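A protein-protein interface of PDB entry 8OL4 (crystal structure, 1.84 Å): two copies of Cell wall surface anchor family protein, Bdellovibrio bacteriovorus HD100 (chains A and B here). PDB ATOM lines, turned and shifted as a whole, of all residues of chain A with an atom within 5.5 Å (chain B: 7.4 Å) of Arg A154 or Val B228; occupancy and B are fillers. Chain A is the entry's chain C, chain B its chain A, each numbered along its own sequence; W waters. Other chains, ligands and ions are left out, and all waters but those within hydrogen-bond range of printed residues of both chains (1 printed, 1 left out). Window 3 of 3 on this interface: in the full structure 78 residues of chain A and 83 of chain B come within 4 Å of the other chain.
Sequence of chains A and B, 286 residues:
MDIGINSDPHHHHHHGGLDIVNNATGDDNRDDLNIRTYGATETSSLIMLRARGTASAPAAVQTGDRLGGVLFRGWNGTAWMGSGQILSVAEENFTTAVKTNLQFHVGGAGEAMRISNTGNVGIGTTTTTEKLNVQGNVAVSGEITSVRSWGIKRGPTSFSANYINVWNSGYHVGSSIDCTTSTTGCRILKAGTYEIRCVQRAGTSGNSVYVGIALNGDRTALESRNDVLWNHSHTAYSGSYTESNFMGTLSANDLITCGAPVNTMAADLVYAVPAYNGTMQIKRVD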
ATOM      1  N   TRP A 150     -13.231  12.667 -12.185  1.00  0.00           N
ATOM      2  CA  TRP A 150     -13.336  11.410 -11.460  1.00  0.00           C
ATOM      3  C   TRP A 150     -14.147  11.642 -10.189  1.00  0.00           C
ATOM      4  O   TRP A 150     -14.315  12.775  -9.728  1.00  0.00           O
ATOM      5  CB  TRP A 150     -11.953  10.825 -11.130  1.00  0.00           C
ATOM      6  CG  TRP A 150     -11.102  11.681 -10.248  1.00  0.00           C
ATOM      7  CD1 TRP A 150     -10.316  12.740 -10.637  1.00  0.00           C
ATOM      8  CD2 TRP A 150     -10.933  11.557  -8.825  1.00  0.00           C
ATOM      9  NE1 TRP A 150      -9.679  13.282  -9.538  1.00  0.00           N
ATOM     10  CE2 TRP A 150     -10.035  12.572  -8.419  1.00  0.00           C
ATOM     11  CE3 TRP A 150     -11.453  10.686  -7.851  1.00  0.00           C
ATOM     12  CZ2 TRP A 150      -9.652  12.749  -7.076  1.00  0.00           C
ATOM     13  CZ3 TRP A 150     -11.060  10.857  -6.515  1.00  0.00           C
ATOM     14  CH2 TRP A 150     -10.174  11.876  -6.145  1.00  0.00           C
ATOM     15  N   ILE A 152     -15.816   9.456  -6.390  1.00  0.00           N
ATOM     16  CA  ILE A 152     -15.799   8.298  -5.505  1.00  0.00           C
ATOM     17  C   ILE A 152     -16.938   8.405  -4.509  1.00  0.00           C
ATOM     18  O   ILE A 152     -17.370   9.504  -4.136  1.00  0.00           O
ATOM     19  CB  ILE A 152     -14.478   8.154  -4.722  1.00  0.00           C
ATOM     20  CG1 ILE A 152     -14.203   9.446  -3.930  1.00  0.00           C
ATOM     21  CG2 ILE A 152     -13.330   7.739  -5.641  1.00  0.00           C
ATOM     22  CD1 ILE A 152     -13.064   9.331  -2.914  1.00  0.00           C
ATOM     23  N   LYS A 153     -17.417   7.241  -4.084  1.00  0.00           N
ATOM     24  CA  LYS A 153     -18.235   7.106  -2.889  1.00  0.00           C
ATOM     25  C   LYS A 153     -17.475   6.248  -1.892  1.00  0.00           C
ATOM     26  O   LYS A 153     -16.751   5.322  -2.282  1.00  0.00           O
ATOM     27  CB  LYS A 153     -19.600   6.465  -3.185  1.00  0.00           C
ATOM     28  CG  LYS A 153     -20.372   7.141  -4.297  1.00  0.00           C
ATOM     29  CD  LYS A 153     -20.738   8.564  -3.908  1.00  0.00           C
ATOM     30  CE  LYS A 153     -21.870   8.583  -2.919  1.00  0.00           C
ATOM     31  NZ  LYS A 153     -22.635   9.872  -2.914  1.00  0.00           N
ATOM     32  N   ARG A 154     -17.670   6.549  -0.605  1.00  0.00           N
ATOM     33  CA  ARG A 154     -16.950   5.904   0.485  1.00  0.00           C
ATOM     34  C   ARG A 154     -17.897   5.556   1.627  1.00  0.00           C
ATOM     35  O   ARG A 154     -18.750   6.371   2.016  1.00  0.00           O
ATOM     36  CB  ARG A 154     -15.827   6.811   1.024  1.00  0.00           C
ATOM     37  CG  ARG A 154     -14.869   7.342  -0.024  1.00  0.00           C
ATOM     38  CD  ARG A 154     -14.019   8.490   0.520  1.00  0.00           C
ATOM     39  NE  ARG A 154     -14.814   9.693   0.759  1.00  0.00           N
ATOM     40  CZ  ARG A 154     -14.338  10.934   0.694  1.00  0.00           C
ATOM     41  NH1 ARG A 154     -13.058  11.149   0.400  1.00  0.00           N
ATOM     42  NH2 ARG A 154     -15.141  11.964   0.931  1.00  0.00           N
ATOM     43  N   GLY A 155     -17.711   4.352   2.183  1.00  0.00           N
ATOM     44  CA  GLY A 155     -18.382   3.942   3.396  1.00  0.00           C
ATOM     45  C   GLY A 155     -19.830   3.547   3.213  1.00  0.00           C
ATOM     46  O   GLY A 155     -20.743   4.350   3.428  1.00  0.00           O
ATOM     47  N   PRO A 156     -20.075   2.293   2.822  1.00  0.00           N
ATOM     48  CA  PRO A 156     -21.470   1.838   2.701  1.00  0.00           C
ATOM     49  C   PRO A 156     -22.113   1.708   4.075  1.00  0.00           C
ATOM     50  O   PRO A 156     -21.726   0.828   4.855  1.00  0.00           O
ATOM     51  CB  PRO A 156     -21.337   0.479   2.006  1.00  0.00           C
ATOM     52  CG  PRO A 156     -19.982  -0.044   2.527  1.00  0.00           C
ATOM     53  CD  PRO A 156     -19.103   1.189   2.689  1.00  0.00           C
ATOM     54  N   TRP A 167     -24.173   5.583   0.827  1.00  0.00           N
ATOM     55  CA  TRP A 167     -22.754   5.784   1.087  1.00  0.00           C
ATOM     56  C   TRP A 167     -22.564   6.975   2.019  1.00  0.00           C
ATOM     57  O   TRP A 167     -23.317   7.957   1.955  1.00  0.00           O
ATOM     58  CB  TRP A 167     -21.974   5.989  -0.215  1.00  0.00           C
ATOM     59  CG  TRP A 167     -22.132   4.842  -1.172  1.00  0.00           C
ATOM     60  CD1 TRP A 167     -23.124   4.683  -2.104  1.00  0.00           C
ATOM     61  CD2 TRP A 167     -21.284   3.684  -1.282  1.00  0.00           C
ATOM     62  NE1 TRP A 167     -22.945   3.497  -2.790  1.00  0.00           N
ATOM     63  CE2 TRP A 167     -21.826   2.865  -2.303  1.00  0.00           C
ATOM     64  CE3 TRP A 167     -20.125   3.255  -0.614  1.00  0.00           C
ATOM     65  CZ2 TRP A 167     -21.244   1.640  -2.675  1.00  0.00           C
ATOM     66  CZ3 TRP A 167     -19.544   2.029  -0.989  1.00  0.00           C
ATOM     67  CH2 TRP A 167     -20.107   1.242  -2.012  1.00  0.00           C
ATOM     68  N   ASN A 168     -21.560   6.908   2.893  1.00  0.00           N
ATOM     69  CA  ASN A 168     -21.370   7.942   3.935  1.00  0.00           C
ATOM     70  C   ASN A 168     -20.845   9.226   3.312  1.00  0.00           C
ATOM     71  O   ASN A 168     -21.255  10.284   3.781  1.00  0.00           O
ATOM     72  CB  ASN A 168     -20.436   7.495   5.049  1.00  0.00           C
ATOM     73  CG  ASN A 168     -20.529   8.395   6.259  1.00  0.00           C
ATOM     74  OD1 ASN A 168     -21.553   8.433   6.930  1.00  0.00           O
ATOM     75  ND2 ASN A 168     -19.470   9.134   6.534  1.00  0.00           N
ATOM     76  N   SER A 169     -19.971   9.135   2.319  1.00  0.00           N
ATOM     77  CA  SER A 169     -19.562  10.397   1.709  1.00  0.00           C
ATOM     78  C   SER A 169     -19.199  10.178   0.251  1.00  0.00           C
ATOM     79  O   SER A 169     -19.043   9.047  -0.211  1.00  0.00           O
ATOM     80  CB  SER A 169     -18.398  11.050   2.466  1.00  0.00           C
ATOM     81  OG  SER A 169     -17.264  10.219   2.432  1.00  0.00           O
ATOM     82  N   GLY A 170     -19.097  11.294  -0.476  1.00  0.00           N
ATOM     83  CA  GLY A 170     -18.642  11.268  -1.848  1.00  0.00           C
ATOM     84  C   GLY A 170     -17.675  12.406  -2.095  1.00  0.00           C
ATOM     85  O   GLY A 170     -17.557  13.339  -1.295  1.00  0.00           O
ATOM     86  N   TYR A 171     -16.977  12.314  -3.220  1.00  0.00           N
ATOM     87  CA  TYR A 171     -16.038  13.363  -3.604  1.00  0.00           C
ATOM     88  C   TYR A 171     -15.857  13.285  -5.110  1.00  0.00           C
ATOM     89  O   TYR A 171     -15.963  12.208  -5.688  1.00  0.00           O
ATOM     90  CB  TYR A 171     -14.681  13.196  -2.885  1.00  0.00           C
ATOM     91  CG  TYR A 171     -13.667  14.252  -3.270  1.00  0.00           C
ATOM     92  CD1 TYR A 171     -13.730  15.528  -2.719  1.00  0.00           C
ATOM     93  CD2 TYR A 171     -12.662  13.985  -4.183  1.00  0.00           C
ATOM     94  CE1 TYR A 171     -12.810  16.507  -3.065  1.00  0.00           C
ATOM     95  CE2 TYR A 171     -11.722  14.963  -4.532  1.00  0.00           C
ATOM     96  CZ  TYR A 171     -11.813  16.216  -3.961  1.00  0.00           C
ATOM     97  OH  TYR A 171     -10.916  17.190  -4.308  1.00  0.00           O
ATOM     98  N   VAL A 273     -18.600   3.158   8.219  1.00  0.00           N
ATOM     99  CA  VAL A 273     -18.149   4.404   7.590  1.00  0.00           C
ATOM    100  C   VAL A 273     -16.781   4.290   6.910  1.00  0.00           C
ATOM    101  O   VAL A 273     -16.619   4.802   5.789  1.00  0.00           O
ATOM    102  CB  VAL A 273     -18.159   5.554   8.613  1.00  0.00           C
ATOM    103  CG1 VAL A 273     -17.417   6.754   8.073  1.00  0.00           C
ATOM    104  CG2 VAL A 273     -19.598   5.944   8.935  1.00  0.00           C
ATOM    105  N   ALA A 275     -13.729   3.874   4.594  1.00  0.00           N
ATOM    106  CA  ALA A 275     -13.765   3.570   3.173  1.00  0.00           C
ATOM    107  C   ALA A 275     -13.255   2.165   2.899  1.00  0.00           C
ATOM    108  O   ALA A 275     -13.654   1.544   1.910  1.00  0.00           O
ATOM    109  CB  ALA A 275     -12.951   4.608   2.391  1.00  0.00           C
ATOM    110  N   GLY A 278     -15.814  -0.358   1.953  1.00  0.00           N
ATOM    111  CA  GLY A 278     -16.357  -0.400   0.613  1.00  0.00           C
ATOM    112  C   GLY A 278     -16.317   0.942  -0.070  1.00  0.00           C
ATOM    113  O   GLY A 278     -16.513   1.982   0.567  1.00  0.00           O
ATOM    114  N   THR A 279     -16.078   0.928  -1.376  1.00  0.00           N
ATOM    115  CA  THR A 279     -15.985   2.163  -2.134  1.00  0.00           C
ATOM    116  C   THR A 279     -16.539   1.946  -3.538  1.00  0.00           C
ATOM    117  O   THR A 279     -16.644   0.815  -4.034  1.00  0.00           O
ATOM    118  CB  THR A 279     -14.533   2.678  -2.252  1.00  0.00           C
ATOM    119  OG1 THR A 279     -13.700   1.672  -2.863  1.00  0.00           O
ATOM    120  CG2 THR A 279     -13.951   3.069  -0.888  1.00  0.00           C
ATOM    121  N   MET A 280     -16.894   3.055  -4.178  1.00  0.00           N
ATOM    122  CA  MET A 280     -17.100   3.073  -5.618  1.00  0.00           C
ATOM    123  C   MET A 280     -16.191   4.141  -6.200  1.00  0.00           C
ATOM    124  O   MET A 280     -16.032   5.214  -5.615  1.00  0.00           O
ATOM    125  CB  MET A 280     -18.567   3.340  -6.008  1.00  0.00           C
ATOM    126  CG  MET A 280     -18.835   3.108  -7.499  1.00  0.00           C
ATOM    127  SD  MET A 280     -20.571   3.176  -8.015  1.00  0.00           S
ATOM    128  CE  MET A 280     -21.361   3.885  -6.580  1.00  0.00           C
ATOM    129  N   ALA B 221      -1.738   9.311   7.025  1.00  0.00           N
ATOM    130  CA  ALA B 221      -1.491  10.511   6.230  1.00  0.00           C
ATOM    131  C   ALA B 221      -2.298  10.506   4.937  1.00  0.00           C
ATOM    132  O   ALA B 221      -2.681  11.570   4.433  1.00  0.00           O
ATOM    133  CB  ALA B 221       0.005  10.647   5.929  1.00  0.00           C
ATOM    134  N   LEU B 222      -2.570   9.330   4.377  1.00  0.00           N
ATOM    135  CA  LEU B 222      -3.416   9.250   3.190  1.00  0.00           C
ATOM    136  C   LEU B 222      -4.870   8.956   3.545  1.00  0.00           C
ATOM    137  O   LEU B 222      -5.783   9.622   3.039  1.00  0.00           O
ATOM    138  CB  LEU B 222      -2.887   8.176   2.225  1.00  0.00           C
ATOM    139  CG  LEU B 222      -1.436   8.284   1.735  1.00  0.00           C
ATOM    140  CD1 LEU B 222      -1.073   7.073   0.856  1.00  0.00           C
ATOM    141  CD2 LEU B 222      -1.165   9.596   0.973  1.00  0.00           C
ATOM    142  N   GLU B 223      -5.099   7.979   4.429  1.00  0.00           N
ATOM    143  CA  GLU B 223      -6.453   7.473   4.654  1.00  0.00           C
ATOM    144  C   GLU B 223      -7.381   8.527   5.252  1.00  0.00           C
ATOM    145  O   GLU B 223      -8.589   8.516   4.981  1.00  0.00           O
ATOM    146  CB  GLU B 223      -6.406   6.243   5.567  1.00  0.00           C
ATOM    147  CG  GLU B 223      -7.743   5.553   5.750  1.00  0.00           C
ATOM    148  CD  GLU B 223      -7.642   4.386   6.699  1.00  0.00           C
ATOM    149  OE1 GLU B 223      -6.684   4.355   7.498  1.00  0.00           O
ATOM    150  OE2 GLU B 223      -8.519   3.496   6.659  1.00  0.00           O
ATOM    151  N   SER B 224      -6.853   9.438   6.067  1.00  0.00           N
ATOM    152  CA  SER B 224      -7.707  10.399   6.757  1.00  0.00           C
ATOM    153  C   SER B 224      -8.116  11.588   5.893  1.00  0.00           C
ATOM    154  O   SER B 224      -8.908  12.408   6.354  1.00  0.00           O
ATOM    155  CB  SER B 224      -7.008  10.900   8.028  1.00  0.00           C
ATOM    156  OG  SER B 224      -5.843  11.648   7.706  1.00  0.00           O
ATOM    157  N   ARG B 225      -7.629  11.700   4.659  1.00  0.00           N
ATOM    158  CA  ARG B 225      -7.936  12.863   3.827  1.00  0.00           C
ATOM    159  C   ARG B 225      -9.342  12.754   3.243  1.00  0.00           C
ATOM    160  O   ARG B 225      -9.762  11.683   2.794  1.00  0.00           O
ATOM    161  CB  ARG B 225      -6.902  12.993   2.706  1.00  0.00           C
ATOM    162  CG  ARG B 225      -5.542  13.535   3.164  1.00  0.00           C
ATOM    163  CD  ARG B 225      -4.491  13.450   2.051  1.00  0.00           C
ATOM    164  NE  ARG B 225      -4.933  14.130   0.833  1.00  0.00           N
ATOM    165  CZ  ARG B 225      -4.324  14.024  -0.347  1.00  0.00           C
ATOM    166  NH1 ARG B 225      -3.227  13.277  -0.474  1.00  0.00           N
ATOM    167  NH2 ARG B 225      -4.806  14.671  -1.398  1.00  0.00           N
ATOM    168  N   ASN B 226     -10.072  13.871   3.247  1.00  0.00           N
ATOM    169  CA  ASN B 226     -11.437  13.860   2.731  1.00  0.00           C
ATOM    170  C   ASN B 226     -11.497  13.929   1.211  1.00  0.00           C
ATOM    171  O   ASN B 226     -12.581  13.760   0.641  1.00  0.00           O
ATOM    172  CB  ASN B 226     -12.256  15.012   3.340  1.00  0.00           C
ATOM    173  CG  ASN B 226     -11.628  16.375   3.107  1.00  0.00           C
ATOM    174  OD1 ASN B 226     -10.872  16.573   2.159  1.00  0.00           O
ATOM    175  ND2 ASN B 226     -11.949  17.331   3.977  1.00  0.00           N
ATOM    176  N   ASP B 227     -10.363  14.144   0.542  1.00  0.00           N
ATOM    177  CA  ASP B 227     -10.331  14.323  -0.906  1.00  0.00           C
ATOM    178  C   ASP B 227      -9.703  13.133  -1.630  1.00  0.00           C
ATOM    179  O   ASP B 227      -9.278  13.261  -2.780  1.00  0.00           O
ATOM    180  CB  ASP B 227      -9.607  15.627  -1.271  1.00  0.00           C
ATOM    181  CG  ASP B 227      -8.152  15.664  -0.798  1.00  0.00           C
ATOM    182  OD1 ASP B 227      -7.833  15.011   0.218  1.00  0.00           O
ATOM    183  OD2 ASP B 227      -7.336  16.381  -1.433  1.00  0.00           O
ATOM    184  N   VAL B 228      -9.645  11.964  -0.994  1.00  0.00           N
ATOM    185  CA  VAL B 228      -9.040  10.805  -1.629  1.00  0.00           C
ATOM    186  C   VAL B 228      -9.892   9.572  -1.386  1.00  0.00           C
ATOM    187  O   VAL B 228     -10.721   9.516  -0.473  1.00  0.00           O
ATOM    188  CB  VAL B 228      -7.601  10.539  -1.140  1.00  0.00           C
ATOM    189  CG1 VAL B 228      -6.774  11.833  -1.159  1.00  0.00           C
ATOM    190  CG2 VAL B 228      -7.620   9.893   0.227  1.00  0.00           C
ATOM    191  N   LEU B 229      -9.668   8.581  -2.229  1.00  0.00           N
ATOM    192  CA  LEU B 229     -10.082   7.216  -1.962  1.00  0.00           C
ATOM    193  C   LEU B 229      -8.897   6.473  -1.369  1.00  0.00           C
ATOM    194  O   LEU B 229      -7.784   6.566  -1.895  1.00  0.00           O
ATOM    195  CB  LEU B 229     -10.535   6.518  -3.245  1.00  0.00           C
ATOM    196  CG  LEU B 229     -10.897   5.031  -3.133  1.00  0.00           C
ATOM    197  CD1 LEU B 229     -11.938   4.670  -4.208  1.00  0.00           C
ATOM    198  CD2 LEU B 229      -9.677   4.138  -3.271  1.00  0.00           C
ATOM    199  N   TRP B 230      -9.146   5.734  -0.294  1.00  0.00           N
ATOM    200  CA  TRP B 230      -8.162   4.833   0.300  1.00  0.00           C
ATOM    201  C   TRP B 230      -8.911   3.620   0.820  1.00  0.00           C
ATOM    202  O   TRP B 230      -9.866   3.766   1.586  1.00  0.00           O
ATOM    203  CB  TRP B 230      -7.387   5.484   1.447  1.00  0.00           C
ATOM    204  CG  TRP B 230      -6.172   4.670   1.871  1.00  0.00           C
ATOM    205  CD1 TRP B 230      -4.874   4.913   1.531  1.00  0.00           C
ATOM    206  CD2 TRP B 230      -6.158   3.485   2.697  1.00  0.00           C
ATOM    207  NE1 TRP B 230      -4.044   3.957   2.095  1.00  0.00           N
ATOM    208  CE2 TRP B 230      -4.809   3.065   2.805  1.00  0.00           C
ATOM    209  CE3 TRP B 230      -7.150   2.734   3.338  1.00  0.00           C
ATOM    210  CZ2 TRP B 230      -4.428   1.934   3.540  1.00  0.00           C
ATOM    211  CZ3 TRP B 230      -6.768   1.600   4.083  1.00  0.00           C
ATOM    212  CH2 TRP B 230      -5.421   1.217   4.179  1.00  0.00           C
ATOM    213  N   ASN B 245      -6.000   0.247  -2.311  1.00  0.00           N
ATOM    214  CA  ASN B 245      -6.154   1.193  -3.420  1.00  0.00           C
ATOM    215  C   ASN B 245      -6.127   2.620  -2.913  1.00  0.00           C
ATOM    216  O   ASN B 245      -6.583   2.911  -1.801  1.00  0.00           O
ATOM    217  CB  ASN B 245      -7.487   1.016  -4.185  1.00  0.00           C
ATOM    218  CG  ASN B 245      -7.625  -0.355  -4.830  1.00  0.00           C
ATOM    219  OD1 ASN B 245      -7.225  -0.557  -5.973  1.00  0.00           O
ATOM    220  ND2 ASN B 245      -8.209  -1.303  -4.090  1.00  0.00           N
ATOM    221  N   PHE B 246      -5.633   3.517  -3.776  1.00  0.00           N
ATOM    222  CA  PHE B 246      -5.616   4.950  -3.518  1.00  0.00           C
ATOM    223  C   PHE B 246      -5.972   5.710  -4.793  1.00  0.00           C
ATOM    224  O   PHE B 246      -5.586   5.316  -5.898  1.00  0.00           O
ATOM    225  CB  PHE B 246      -4.233   5.424  -3.034  1.00  0.00           C
ATOM    226  CG  PHE B 246      -4.117   6.920  -2.898  1.00  0.00           C
ATOM    227  CD1 PHE B 246      -4.451   7.548  -1.696  1.00  0.00           C
ATOM    228  CD2 PHE B 246      -3.665   7.696  -3.957  1.00  0.00           C
ATOM    229  CE1 PHE B 246      -4.342   8.922  -1.562  1.00  0.00           C
ATOM    230  CE2 PHE B 246      -3.547   9.069  -3.832  1.00  0.00           C
ATOM    231  CZ  PHE B 246      -3.883   9.686  -2.646  1.00  0.00           C
ATOM    232  N   MET B 247      -6.698   6.809  -4.626  1.00  0.00           N
ATOM    233  CA  MET B 247      -6.964   7.716  -5.741  1.00  0.00           C
ATOM    234  C   MET B 247      -6.993   9.128  -5.189  1.00  0.00           C
ATOM    235  O   MET B 247      -7.757   9.394  -4.255  1.00  0.00           O
ATOM    236  CB  MET B 247      -8.291   7.371  -6.428  1.00  0.00           C
ATOM    237  CG  MET B 247      -8.715   8.357  -7.507  1.00  0.00           C
ATOM    238  SD  MET B 247      -7.704   8.234  -8.995  1.00  0.00           S
ATOM    239  CE  MET B 247      -8.718   7.189 -10.018  1.00  0.00           C
ATOM    240  N   GLY B 248      -6.170  10.018  -5.731  1.00  0.00           N
ATOM    241  CA  GLY B 248      -6.222  11.404  -5.303  1.00  0.00           C
ATOM    242  C   GLY B 248      -4.919  12.138  -5.544  1.00  0.00           C
ATOM    243  O   GLY B 248      -3.971  11.597  -6.105  1.00  0.00           O
ATOM    244  N   THR B 249      -4.888  13.391  -5.090  1.00  0.00           N
ATOM    245  CA  THR B 249      -3.713  14.220  -5.341  1.00  0.00           C
ATOM    246  C   THR B 249      -2.580  13.872  -4.388  1.00  0.00           C
ATOM    247  O   THR B 249      -2.800  13.449  -3.249  1.00  0.00           O
ATOM    248  CB  THR B 249      -4.034  15.709  -5.223  1.00  0.00           C
ATOM    249  OG1 THR B 249      -4.552  15.996  -3.919  1.00  0.00           O
ATOM    250  CG2 THR B 249      -5.032  16.141  -6.308  1.00  0.00           C
ATOM    251  N   LEU B 250      -1.356  14.026  -4.889  1.00  0.00           N
ATOM    252  CA  LEU B 250      -0.143  13.875  -4.104  1.00  0.00           C
ATOM    253  C   LEU B 250       0.827  15.004  -4.448  1.00  0.00           C
ATOM    254  O   LEU B 250       0.777  15.611  -5.537  1.00  0.00           O
ATOM    255  CB  LEU B 250       0.526  12.510  -4.345  1.00  0.00           C
ATOM    256  CG  LEU B 250      -0.300  11.269  -3.982  1.00  0.00           C
ATOM    257  CD1 LEU B 250       0.332  10.019  -4.581  1.00  0.00           C
ATOM    258  CD2 LEU B 250      -0.437  11.141  -2.467  1.00  0.00           C
HETATM  259  O   HOH W   1     -10.443   3.641   4.810  1.00  0.00           O
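No position is printed for both chains.
Of the 10 pairs that touch across the chains among the printed residues, none has its exchanged pair printed and touching as well.
Of the printed residues of chain B, Arg A154 touches Asn B226 and Val B228.
Printed residues of chain B within 4 Å of Ala A275: Trp B230.
Of the printed residues of chain A, Asp B227 touches Trp A150 (3.7 Å) and Tyr A171 (3.5 Å).
Of the printed residues of chain A, Val B228 touches Ile A152 and Arg A154.
Among the printed residues, pairs that only touch across the chains: Trp A150 with Asp B227 (3.7 Å), Trp A150 with Met B247 (3.6 Å), Ile A152 with Val B228 (3.4 Å), Ile A152 with Leu B229 (3.5 Å), Tyr A171 with Asn B226 (3.97 Å), Tyr A171 with Asp B227 (3.5 Å), Ala A275 with Trp B230 (3.3 Å) and Thr A279 with Leu B229 (3.7 Å).
The backbone carbonyl oxygen (O) of Asn B226 lies within hydrogen-bond range of the guanidinium group (NH1) of Arg A154 (2.7 Å).
O of Val B228 lies within hydrogen-bond range of NH1 of Arg A154 (3.0 Å).
O of Tyr A171 sits at hydrogen-bond distance from N of Ile A152 (2.8 Å).
The side-chain carboxylate (OD2) of Asp B227 lies within salt-bridge range of the guanidinium group (NH2) of Arg B225 (3.1 Å).
The backbone carbonyl oxygen of Ser A169 sits at hydrogen-bond distance from the backbone NH of Arg A154 (2.9 Å).
The backbone carbonyl oxygen of Met B247 lies within hydrogen-bond range of the backbone NH of Leu B229.
O of Arg A154 is in hydrogen-bond range of N of Asn A168, 3.0 Å away.
Printed residues of chain A that touch a printed residue of chain B: Trp A150, Ile A152, Arg A154, Tyr A171, Ala A275 and Thr A279.
Hydrophobic or aromatic side chains of chain A that line the printed part of chain B: Trp A150, Ile A152, Tyr A171 and Ala A275.
Along chain A the printed residues that touch a printed residue of chain B span positions 150 to 279.
Of the 16 printed residues of chain B, 6 touch a printed residue of chain A.
Among the printed residues, 10 pairs touch across the chains.
Among the printed residues, no Asp or Glu carboxylate lies within 4 Å of a Lys or Arg side-chain nitrogen of the other chain.
Water W1 lies within hydrogen-bond range of the side-chain carboxylate of Glu B223 (2.7 Å), the backbone carbonyl oxygen of Trp B230 (3.3 Å) and the backbone NH of Ala A275 (3.3 Å).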
